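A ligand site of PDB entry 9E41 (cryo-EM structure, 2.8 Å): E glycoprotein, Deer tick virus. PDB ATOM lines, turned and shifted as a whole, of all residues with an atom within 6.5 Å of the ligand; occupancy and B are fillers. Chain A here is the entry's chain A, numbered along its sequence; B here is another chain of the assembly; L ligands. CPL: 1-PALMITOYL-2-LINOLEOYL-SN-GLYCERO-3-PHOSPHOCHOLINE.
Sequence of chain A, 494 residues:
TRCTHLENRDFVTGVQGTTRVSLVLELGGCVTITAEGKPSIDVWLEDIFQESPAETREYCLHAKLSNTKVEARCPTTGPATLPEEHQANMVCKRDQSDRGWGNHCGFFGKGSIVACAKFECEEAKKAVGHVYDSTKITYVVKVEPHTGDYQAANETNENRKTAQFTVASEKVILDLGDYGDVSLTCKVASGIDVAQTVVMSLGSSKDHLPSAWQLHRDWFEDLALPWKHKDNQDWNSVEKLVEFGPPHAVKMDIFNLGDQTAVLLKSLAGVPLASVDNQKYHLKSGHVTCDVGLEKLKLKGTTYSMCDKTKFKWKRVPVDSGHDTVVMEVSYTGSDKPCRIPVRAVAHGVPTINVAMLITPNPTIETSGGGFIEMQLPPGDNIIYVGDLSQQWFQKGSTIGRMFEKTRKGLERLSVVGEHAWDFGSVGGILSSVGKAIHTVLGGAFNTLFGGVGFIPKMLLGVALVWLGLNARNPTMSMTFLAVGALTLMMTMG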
ATOM      1  N   LEU A 411      -6.448  17.098  16.871  1.00  0.00           N
ATOM      2  CA  LEU A 411      -7.655  16.837  17.651  1.00  0.00           C
ATOM      3  C   LEU A 411      -8.347  15.562  17.190  1.00  0.00           C
ATOM      4  O   LEU A 411      -8.843  14.775  18.012  1.00  0.00           O
ATOM      5  CB  LEU A 411      -8.610  18.022  17.535  1.00  0.00           C
ATOM      6  CG  LEU A 411      -8.133  19.338  18.146  1.00  0.00           C
ATOM      7  CD1 LEU A 411      -9.092  20.461  17.793  1.00  0.00           C
ATOM      8  CD2 LEU A 411      -8.001  19.232  19.654  1.00  0.00           C
ATOM      9  N   GLU A 412      -8.413  15.337  15.878  1.00  0.00           N
ATOM     10  CA  GLU A 412      -9.062  14.136  15.360  1.00  0.00           C
ATOM     11  C   GLU A 412      -8.279  12.879  15.725  1.00  0.00           C
ATOM     12  O   GLU A 412      -8.868  11.857  16.074  1.00  0.00           O
ATOM     13  CB  GLU A 412      -9.241  14.259  13.854  1.00  0.00           C
ATOM     14  CG  GLU A 412      -9.663  12.980  13.142  1.00  0.00           C
ATOM     15  CD  GLU A 412      -9.563  13.092  11.638  1.00  0.00           C
ATOM     16  OE1 GLU A 412     -10.114  14.064  11.067  1.00  0.00           O
ATOM     17  OE2 GLU A 412      -8.924  12.215  11.015  1.00  0.00           O
ATOM     18  N   ARG A 413      -6.946  12.943  15.652  1.00  0.00           N
ATOM     19  CA  ARG A 413      -6.134  11.826  16.113  1.00  0.00           C
ATOM     20  C   ARG A 413      -6.364  11.556  17.586  1.00  0.00           C
ATOM     21  O   ARG A 413      -6.464  10.399  18.015  1.00  0.00           O
ATOM     22  CB  ARG A 413      -4.651  12.090  15.849  1.00  0.00           C
ATOM     23  CG  ARG A 413      -3.733  11.118  16.570  1.00  0.00           C
ATOM     24  CD  ARG A 413      -2.402  10.977  15.858  1.00  0.00           C
ATOM     25  NE  ARG A 413      -1.830  12.271  15.511  1.00  0.00           N
ATOM     26  CZ  ARG A 413      -1.855  12.816  14.299  1.00  0.00           C
ATOM     27  NH1 ARG A 413      -2.438  12.203  13.281  1.00  0.00           N
ATOM     28  NH2 ARG A 413      -1.294  13.997  14.103  1.00  0.00           N
ATOM     29  N   LEU A 414      -6.454  12.619  18.385  1.00  0.00           N
ATOM     30  CA  LEU A 414      -6.725  12.466  19.813  1.00  0.00           C
ATOM     31  C   LEU A 414      -8.084  11.820  20.052  1.00  0.00           C
ATOM     32  O   LEU A 414      -8.251  10.983  20.943  1.00  0.00           O
ATOM     33  CB  LEU A 414      -6.641  13.831  20.500  1.00  0.00           C
ATOM     34  CG  LEU A 414      -6.467  13.906  22.014  1.00  0.00           C
ATOM     35  CD1 LEU A 414      -5.251  13.126  22.475  1.00  0.00           C
ATOM     36  CD2 LEU A 414      -6.369  15.356  22.442  1.00  0.00           C
ATOM     37  N   SER A 415      -9.079  12.191  19.245  1.00  0.00           N
ATOM     38  CA  SER A 415     -10.427  11.655  19.408  1.00  0.00           C
ATOM     39  C   SER A 415     -10.481  10.181  18.999  1.00  0.00           C
ATOM     40  O   SER A 415     -11.191   9.395  19.633  1.00  0.00           O
ATOM     41  CB  SER A 415     -11.417  12.465  18.580  1.00  0.00           C
ATOM     42  OG  SER A 415     -12.613  11.737  18.358  1.00  0.00           O
ATOM     43  N   VAL A 416      -9.753   9.803  17.957  1.00  0.00           N
ATOM     44  CA  VAL A 416      -9.839   8.455  17.413  1.00  0.00           C
ATOM     45  C   VAL A 416      -8.939   7.521  18.211  1.00  0.00           C
ATOM     46  O   VAL A 416      -9.414   6.582  18.853  1.00  0.00           O
ATOM     47  CB  VAL A 416      -9.460   8.435  15.928  1.00  0.00           C
ATOM     48  CG1 VAL A 416      -9.094   7.028  15.480  1.00  0.00           C
ATOM     49  CG2 VAL A 416     -10.599   8.987  15.083  1.00  0.00           C
ATOM     50  N   VAL A 417      -7.633   7.770  18.177  1.00  0.00           N
ATOM     51  CA  VAL A 417      -6.672   6.841  18.779  1.00  0.00           C
ATOM     52  C   VAL A 417      -6.763   6.883  20.296  1.00  0.00           C
ATOM     53  O   VAL A 417      -6.898   5.848  20.960  1.00  0.00           O
ATOM     54  CB  VAL A 417      -5.245   7.153  18.285  1.00  0.00           C
ATOM     55  CG1 VAL A 417      -4.236   6.349  19.065  1.00  0.00           C
ATOM     56  CG2 VAL A 417      -5.124   6.858  16.806  1.00  0.00           C
ATOM     57  N   GLY A 418      -6.698   8.079  20.884  1.00  0.00           N
ATOM     58  CA  GLY A 418      -6.777   8.231  22.325  1.00  0.00           C
ATOM     59  C   GLY A 418      -5.456   8.637  22.957  1.00  0.00           C
ATOM     60  O   GLY A 418      -4.741   9.485  22.425  1.00  0.00           O
ATOM     61  N   GLU A 419      -5.129   8.030  24.105  1.00  0.00           N
ATOM     62  CA  GLU A 419      -3.940   8.434  24.839  1.00  0.00           C
ATOM     63  C   GLU A 419      -2.661   8.196  24.057  1.00  0.00           C
ATOM     64  O   GLU A 419      -1.648   8.859  24.336  1.00  0.00           O
ATOM     65  CB  GLU A 419      -3.874   7.683  26.176  1.00  0.00           C
ATOM     66  CG  GLU A 419      -3.682   6.188  26.057  1.00  0.00           C
ATOM     67  CD  GLU A 419      -3.659   5.495  27.399  1.00  0.00           C
ATOM     68  OE1 GLU A 419      -3.828   6.182  28.432  1.00  0.00           O
ATOM     69  OE2 GLU A 419      -3.486   4.254  27.437  1.00  0.00           O
ATOM     70  N   TRP A 422      -0.322  11.006  22.074  1.00  0.00           N
ATOM     71  CA  TRP A 422       0.849  11.686  22.599  1.00  0.00           C
ATOM     72  C   TRP A 422       2.143  10.953  22.279  1.00  0.00           C
ATOM     73  O   TRP A 422       3.222  11.489  22.542  1.00  0.00           O
ATOM     74  CB  TRP A 422       0.716  11.854  24.112  1.00  0.00           C
ATOM     75  CG  TRP A 422      -0.528  12.599  24.506  1.00  0.00           C
ATOM     76  CD1 TRP A 422      -1.732  12.047  24.818  1.00  0.00           C
ATOM     77  CD2 TRP A 422      -0.676  14.010  24.635  1.00  0.00           C
ATOM     78  NE1 TRP A 422      -2.628  13.036  25.129  1.00  0.00           N
ATOM     79  CE2 TRP A 422      -2.010  14.256  25.022  1.00  0.00           C
ATOM     80  CE3 TRP A 422       0.180  15.102  24.460  1.00  0.00           C
ATOM     81  CZ2 TRP A 422      -2.499  15.537  25.244  1.00  0.00           C
ATOM     82  CZ3 TRP A 422      -0.318  16.374  24.673  1.00  0.00           C
ATOM     83  CH2 TRP A 422      -1.645  16.578  25.061  1.00  0.00           C
ATOM     84  N   GLY A 435       0.745  15.149  29.726  1.00  0.00           N
ATOM     85  CA  GLY A 435      -0.489  15.128  28.967  1.00  0.00           C
ATOM     86  C   GLY A 435      -1.069  13.738  28.861  1.00  0.00           C
ATOM     87  O   GLY A 435      -2.279  13.552  28.981  1.00  0.00           O
ATOM     88  N   ILE A 438      -2.628  12.802  32.246  1.00  0.00           N
ATOM     89  CA  ILE A 438      -3.873  13.526  32.445  1.00  0.00           C
ATOM     90  C   ILE A 438      -4.982  12.938  31.582  1.00  0.00           C
ATOM     91  O   ILE A 438      -6.118  12.723  32.039  1.00  0.00           O
ATOM     92  CB  ILE A 438      -3.676  15.025  32.156  1.00  0.00           C
ATOM     93  CG1 ILE A 438      -2.789  15.642  33.235  1.00  0.00           C
ATOM     94  CG2 ILE A 438      -5.021  15.718  32.066  1.00  0.00           C
ATOM     95  CD1 ILE A 438      -2.269  17.020  32.874  1.00  0.00           C
ATOM     96  N   HIS A 439      -4.681  12.663  30.314  1.00  0.00           N
ATOM     97  CA  HIS A 439      -5.683  12.094  29.415  1.00  0.00           C
ATOM     98  C   HIS A 439      -6.090  10.699  29.856  1.00  0.00           C
ATOM     99  O   HIS A 439      -7.257  10.321  29.732  1.00  0.00           O
ATOM    100  CB  HIS A 439      -5.170  12.079  27.981  1.00  0.00           C
ATOM    101  CG  HIS A 439      -6.191  11.646  26.984  1.00  0.00           C
ATOM    102  ND1 HIS A 439      -6.444  10.317  26.700  1.00  0.00           N
ATOM    103  CD2 HIS A 439      -7.033  12.358  26.203  1.00  0.00           C
ATOM    104  CE1 HIS A 439      -7.395  10.239  25.792  1.00  0.00           C
ATOM    105  NE2 HIS A 439      -7.777  11.460  25.474  1.00  0.00           N
ATOM    106  N   LEU A 442      -8.487  11.197  32.806  1.00  0.00           N
ATOM    107  CA  LEU A 442      -9.766  11.726  32.324  1.00  0.00           C
ATOM    108  C   LEU A 442     -10.549  10.664  31.570  1.00  0.00           C
ATOM    109  O   LEU A 442     -11.769  10.531  31.754  1.00  0.00           O
ATOM    110  CB  LEU A 442      -9.530  12.947  31.432  1.00  0.00           C
ATOM    111  CG  LEU A 442      -8.994  14.220  32.091  1.00  0.00           C
ATOM    112  CD1 LEU A 442      -8.989  15.347  31.078  1.00  0.00           C
ATOM    113  CD2 LEU A 442      -9.809  14.615  33.320  1.00  0.00           C
ATOM    114  N   GLY A 443      -9.877   9.911  30.702  1.00  0.00           N
ATOM    115  CA  GLY A 443     -10.546   8.850  29.974  1.00  0.00           C
ATOM    116  C   GLY A 443     -11.060   7.759  30.883  1.00  0.00           C
ATOM    117  O   GLY A 443     -12.142   7.209  30.663  1.00  0.00           O
ATOM    118  N   GLY A 444     -10.291   7.414  31.915  1.00  0.00           N
ATOM    119  CA  GLY A 444     -10.760   6.429  32.868  1.00  0.00           C
ATOM    120  C   GLY A 444     -12.027   6.872  33.572  1.00  0.00           C
ATOM    121  O   GLY A 444     -12.992   6.114  33.700  1.00  0.00           O
ATOM    122  N   PHE A 446     -14.213   9.134  32.496  1.00  0.00           N
ATOM    123  CA  PHE A 446     -15.300   9.211  31.532  1.00  0.00           C
ATOM    124  C   PHE A 446     -15.827   7.834  31.166  1.00  0.00           C
ATOM    125  O   PHE A 446     -17.037   7.663  30.979  1.00  0.00           O
ATOM    126  CB  PHE A 446     -14.814   9.954  30.289  1.00  0.00           C
ATOM    127  CG  PHE A 446     -15.916  10.388  29.360  1.00  0.00           C
ATOM    128  CD1 PHE A 446     -16.370   9.558  28.358  1.00  0.00           C
ATOM    129  CD2 PHE A 446     -16.496  11.632  29.510  1.00  0.00           C
ATOM    130  CE1 PHE A 446     -17.385   9.961  27.513  1.00  0.00           C
ATOM    131  CE2 PHE A 446     -17.517  12.042  28.675  1.00  0.00           C
ATOM    132  CZ  PHE A 446     -17.956  11.205  27.667  1.00  0.00           C
ATOM    133  N   LEU A 489     -18.994  17.675  28.027  1.00  0.00           N
ATOM    134  CA  LEU A 489     -19.406  18.103  26.695  1.00  0.00           C
ATOM    135  C   LEU A 489     -18.279  17.944  25.694  1.00  0.00           C
ATOM    136  O   LEU A 489     -18.497  17.478  24.567  1.00  0.00           O
ATOM    137  CB  LEU A 489     -19.863  19.559  26.740  1.00  0.00           C
ATOM    138  CG  LEU A 489     -21.251  19.863  27.326  1.00  0.00           C
ATOM    139  CD1 LEU A 489     -21.478  21.363  27.388  1.00  0.00           C
ATOM    140  CD2 LEU A 489     -22.349  19.182  26.524  1.00  0.00           C
ATOM    141  N   MET A 490     -17.062  18.313  26.084  1.00  0.00           N
ATOM    142  CA  MET A 490     -15.915  18.209  25.178  1.00  0.00           C
ATOM    143  C   MET A 490     -15.616  16.754  24.831  1.00  0.00           C
ATOM    144  O   MET A 490     -15.369  16.433  23.661  1.00  0.00           O
ATOM    145  CB  MET A 490     -14.706  18.879  25.812  1.00  0.00           C
ATOM    146  CG  MET A 490     -14.699  20.389  25.704  1.00  0.00           C
ATOM    147  SD  MET A 490     -13.516  21.142  26.826  1.00  0.00           S
ATOM    148  CE  MET A 490     -13.560  22.847  26.295  1.00  0.00           C
ATOM    149  N   MET A 491     -15.638  15.865  25.822  1.00  0.00           N
ATOM    150  CA  MET A 491     -15.359  14.456  25.554  1.00  0.00           C
ATOM    151  C   MET A 491     -16.501  13.817  24.775  1.00  0.00           C
ATOM    152  O   MET A 491     -16.282  12.850  24.034  1.00  0.00           O
ATOM    153  CB  MET A 491     -15.137  13.713  26.870  1.00  0.00           C
ATOM    154  CG  MET A 491     -13.871  14.091  27.607  1.00  0.00           C
ATOM    155  SD  MET A 491     -12.376  13.585  26.727  1.00  0.00           S
ATOM    156  CE  MET A 491     -11.110  14.324  27.748  1.00  0.00           C
ATOM    157  N   THR A 492     -17.718  14.327  24.925  1.00  0.00           N
ATOM    158  CA  THR A 492     -18.875  13.666  24.341  1.00  0.00           C
ATOM    159  C   THR A 492     -18.851  13.735  22.821  1.00  0.00           C
ATOM    160  O   THR A 492     -19.248  12.783  22.147  1.00  0.00           O
ATOM    161  CB  THR A 492     -20.160  14.299  24.879  1.00  0.00           C
ATOM    162  OG1 THR A 492     -20.121  14.326  26.313  1.00  0.00           O
ATOM    163  CG2 THR A 492     -21.375  13.518  24.425  1.00  0.00           C
ATOM    164  N   MET A 493     -18.394  14.856  22.261  1.00  0.00           N
ATOM    165  CA  MET A 493     -18.368  15.008  20.811  1.00  0.00           C
ATOM    166  C   MET A 493     -17.475  13.950  20.160  1.00  0.00           C
ATOM    167  O   MET A 493     -17.838  13.366  19.134  1.00  0.00           O
ATOM    168  CB  MET A 493     -17.909  16.413  20.420  1.00  0.00           C
ATOM    169  CG  MET A 493     -18.596  17.534  21.190  1.00  0.00           C
ATOM    170  SD  MET A 493     -20.393  17.493  21.046  1.00  0.00           S
ATOM    171  CE  MET A 493     -20.794  19.231  21.208  1.00  0.00           C
ATOM    172  N   GLY A 494     -16.313  13.682  20.751  1.00  0.00           N
ATOM    173  CA  GLY A 494     -15.409  12.677  20.228  1.00  0.00           C
ATOM    174  C   GLY A 494     -16.030  11.298  20.174  1.00  0.00           C
ATOM    175  O   GLY A 494     -16.698  10.945  19.210  1.00  0.00           O
ATOM    176  N   ASP B  11     -15.335   2.120  21.993  1.00  0.00           N
ATOM    177  CA  ASP B  11     -13.924   1.950  22.308  1.00  0.00           C
ATOM    178  C   ASP B  11     -13.141   1.258  21.210  1.00  0.00           C
ATOM    179  O   ASP B  11     -11.908   1.206  21.279  1.00  0.00           O
ATOM    180  CB  ASP B  11     -13.771   1.154  23.610  1.00  0.00           C
ATOM    181  CG  ASP B  11     -14.277   1.914  24.825  1.00  0.00           C
ATOM    182  OD1 ASP B  11     -14.219   3.155  24.812  1.00  0.00           O
ATOM    183  OD2 ASP B  11     -14.726   1.264  25.790  1.00  0.00           O
HETATM  184  C1  CPL L   1     -11.937  15.159  23.277  1.00  0.00           C
HETATM  185  C2  CPL L   1     -11.219  16.352  22.689  1.00  0.00           C
HETATM  186  C3  CPL L   1      -9.705  16.298  22.701  1.00  0.00           C
HETATM  187  C4  CPL L   1     -11.449  10.695  23.357  1.00  0.00           C
HETATM  188  C5  CPL L   1     -10.524   9.751  24.093  1.00  0.00           C
HETATM  189  C6  CPL L   1     -12.498   8.878  25.285  1.00  0.00           C
HETATM  190  C7  CPL L   1     -10.320   7.824  25.519  1.00  0.00           C
HETATM  191  C8  CPL L   1     -10.730   9.977  26.553  1.00  0.00           C
HETATM  192  C11 CPL L   1      -9.238  17.452  24.694  1.00  0.00           C
HETATM  193  C12 CPL L   1      -8.073  17.601  25.630  1.00  0.00           C
HETATM  194  C13 CPL L   1      -7.467  16.298  26.126  1.00  0.00           C
HETATM  195  C14 CPL L   1      -6.130  16.519  26.813  1.00  0.00           C
HETATM  196  C15 CPL L   1      -6.150  16.089  28.276  1.00  0.00           C
HETATM  197  C31 CPL L   1     -12.629  17.492  21.162  1.00  0.00           C
HETATM  198  C32 CPL L   1     -12.667  17.985  19.748  1.00  0.00           C
HETATM  199  C33 CPL L   1     -13.781  18.987  19.472  1.00  0.00           C
HETATM  200  C34 CPL L   1     -13.709  20.206  20.384  1.00  0.00           C
HETATM  201  C35 CPL L   1     -12.476  21.065  20.142  1.00  0.00           C
HETATM  202  N   CPL L   1     -11.037   9.124  25.363  1.00  0.00           N
HETATM  203  O2  CPL L   1     -11.637  16.612  21.353  1.00  0.00           O
HETATM  204  O3  CPL L   1      -9.204  16.310  24.030  1.00  0.00           O
HETATM  205  O11 CPL L   1     -10.111  18.275  24.547  1.00  0.00           O
HETATM  206  O31 CPL L   1     -13.390  17.815  22.036  1.00  0.00           O
HETATM  207  O1P CPL L   1      -9.395  12.419  22.721  1.00  0.00           O
HETATM  208  O2P CPL L   1      -9.980  13.828  24.814  1.00  0.00           O
HETATM  209  O3P CPL L   1     -11.465  13.956  22.712  1.00  0.00           O
HETATM  210  O4P CPL L   1     -11.545  11.943  24.009  1.00  0.00           O
HETATM  211  P   CPL L   1     -10.420  13.074  23.611  1.00  0.00           P
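O of Met 490 lies close to O31 of the ligand (2.9 Å). Residues that only touch the ligand: Ile 438 (3.97 Å) and Gly 443 (3.6 Å). Hydrophobic or aromatic side chains that line the ligand: Leu 414, Ile 438, His 439 and Met 491. Within 4 Å of the ligand: Leu 414, Ser 415, Ile 438, His 439, Gly 443, Met 490 and Met 491. Along chain A the residues within 4 Å of the ligand span positions 414 to 491. The nearest printed residue that does not touch the ligand is Leu 442 (4.1 Å).
O1P of the ligand lies close to O of Leu 414, 2.6 Å away. The side-chain sulfur (SD) of Met 491 lies close to an oxygen (O2P) of the ligand. NE2 of His 439 is in hydrogen-bond range of O2P of the ligand, at 3.3 Å. An oxygen (O1P) of the ligand sits at hydrogen-bond distance from the backbone NH (N) of Ser 415.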
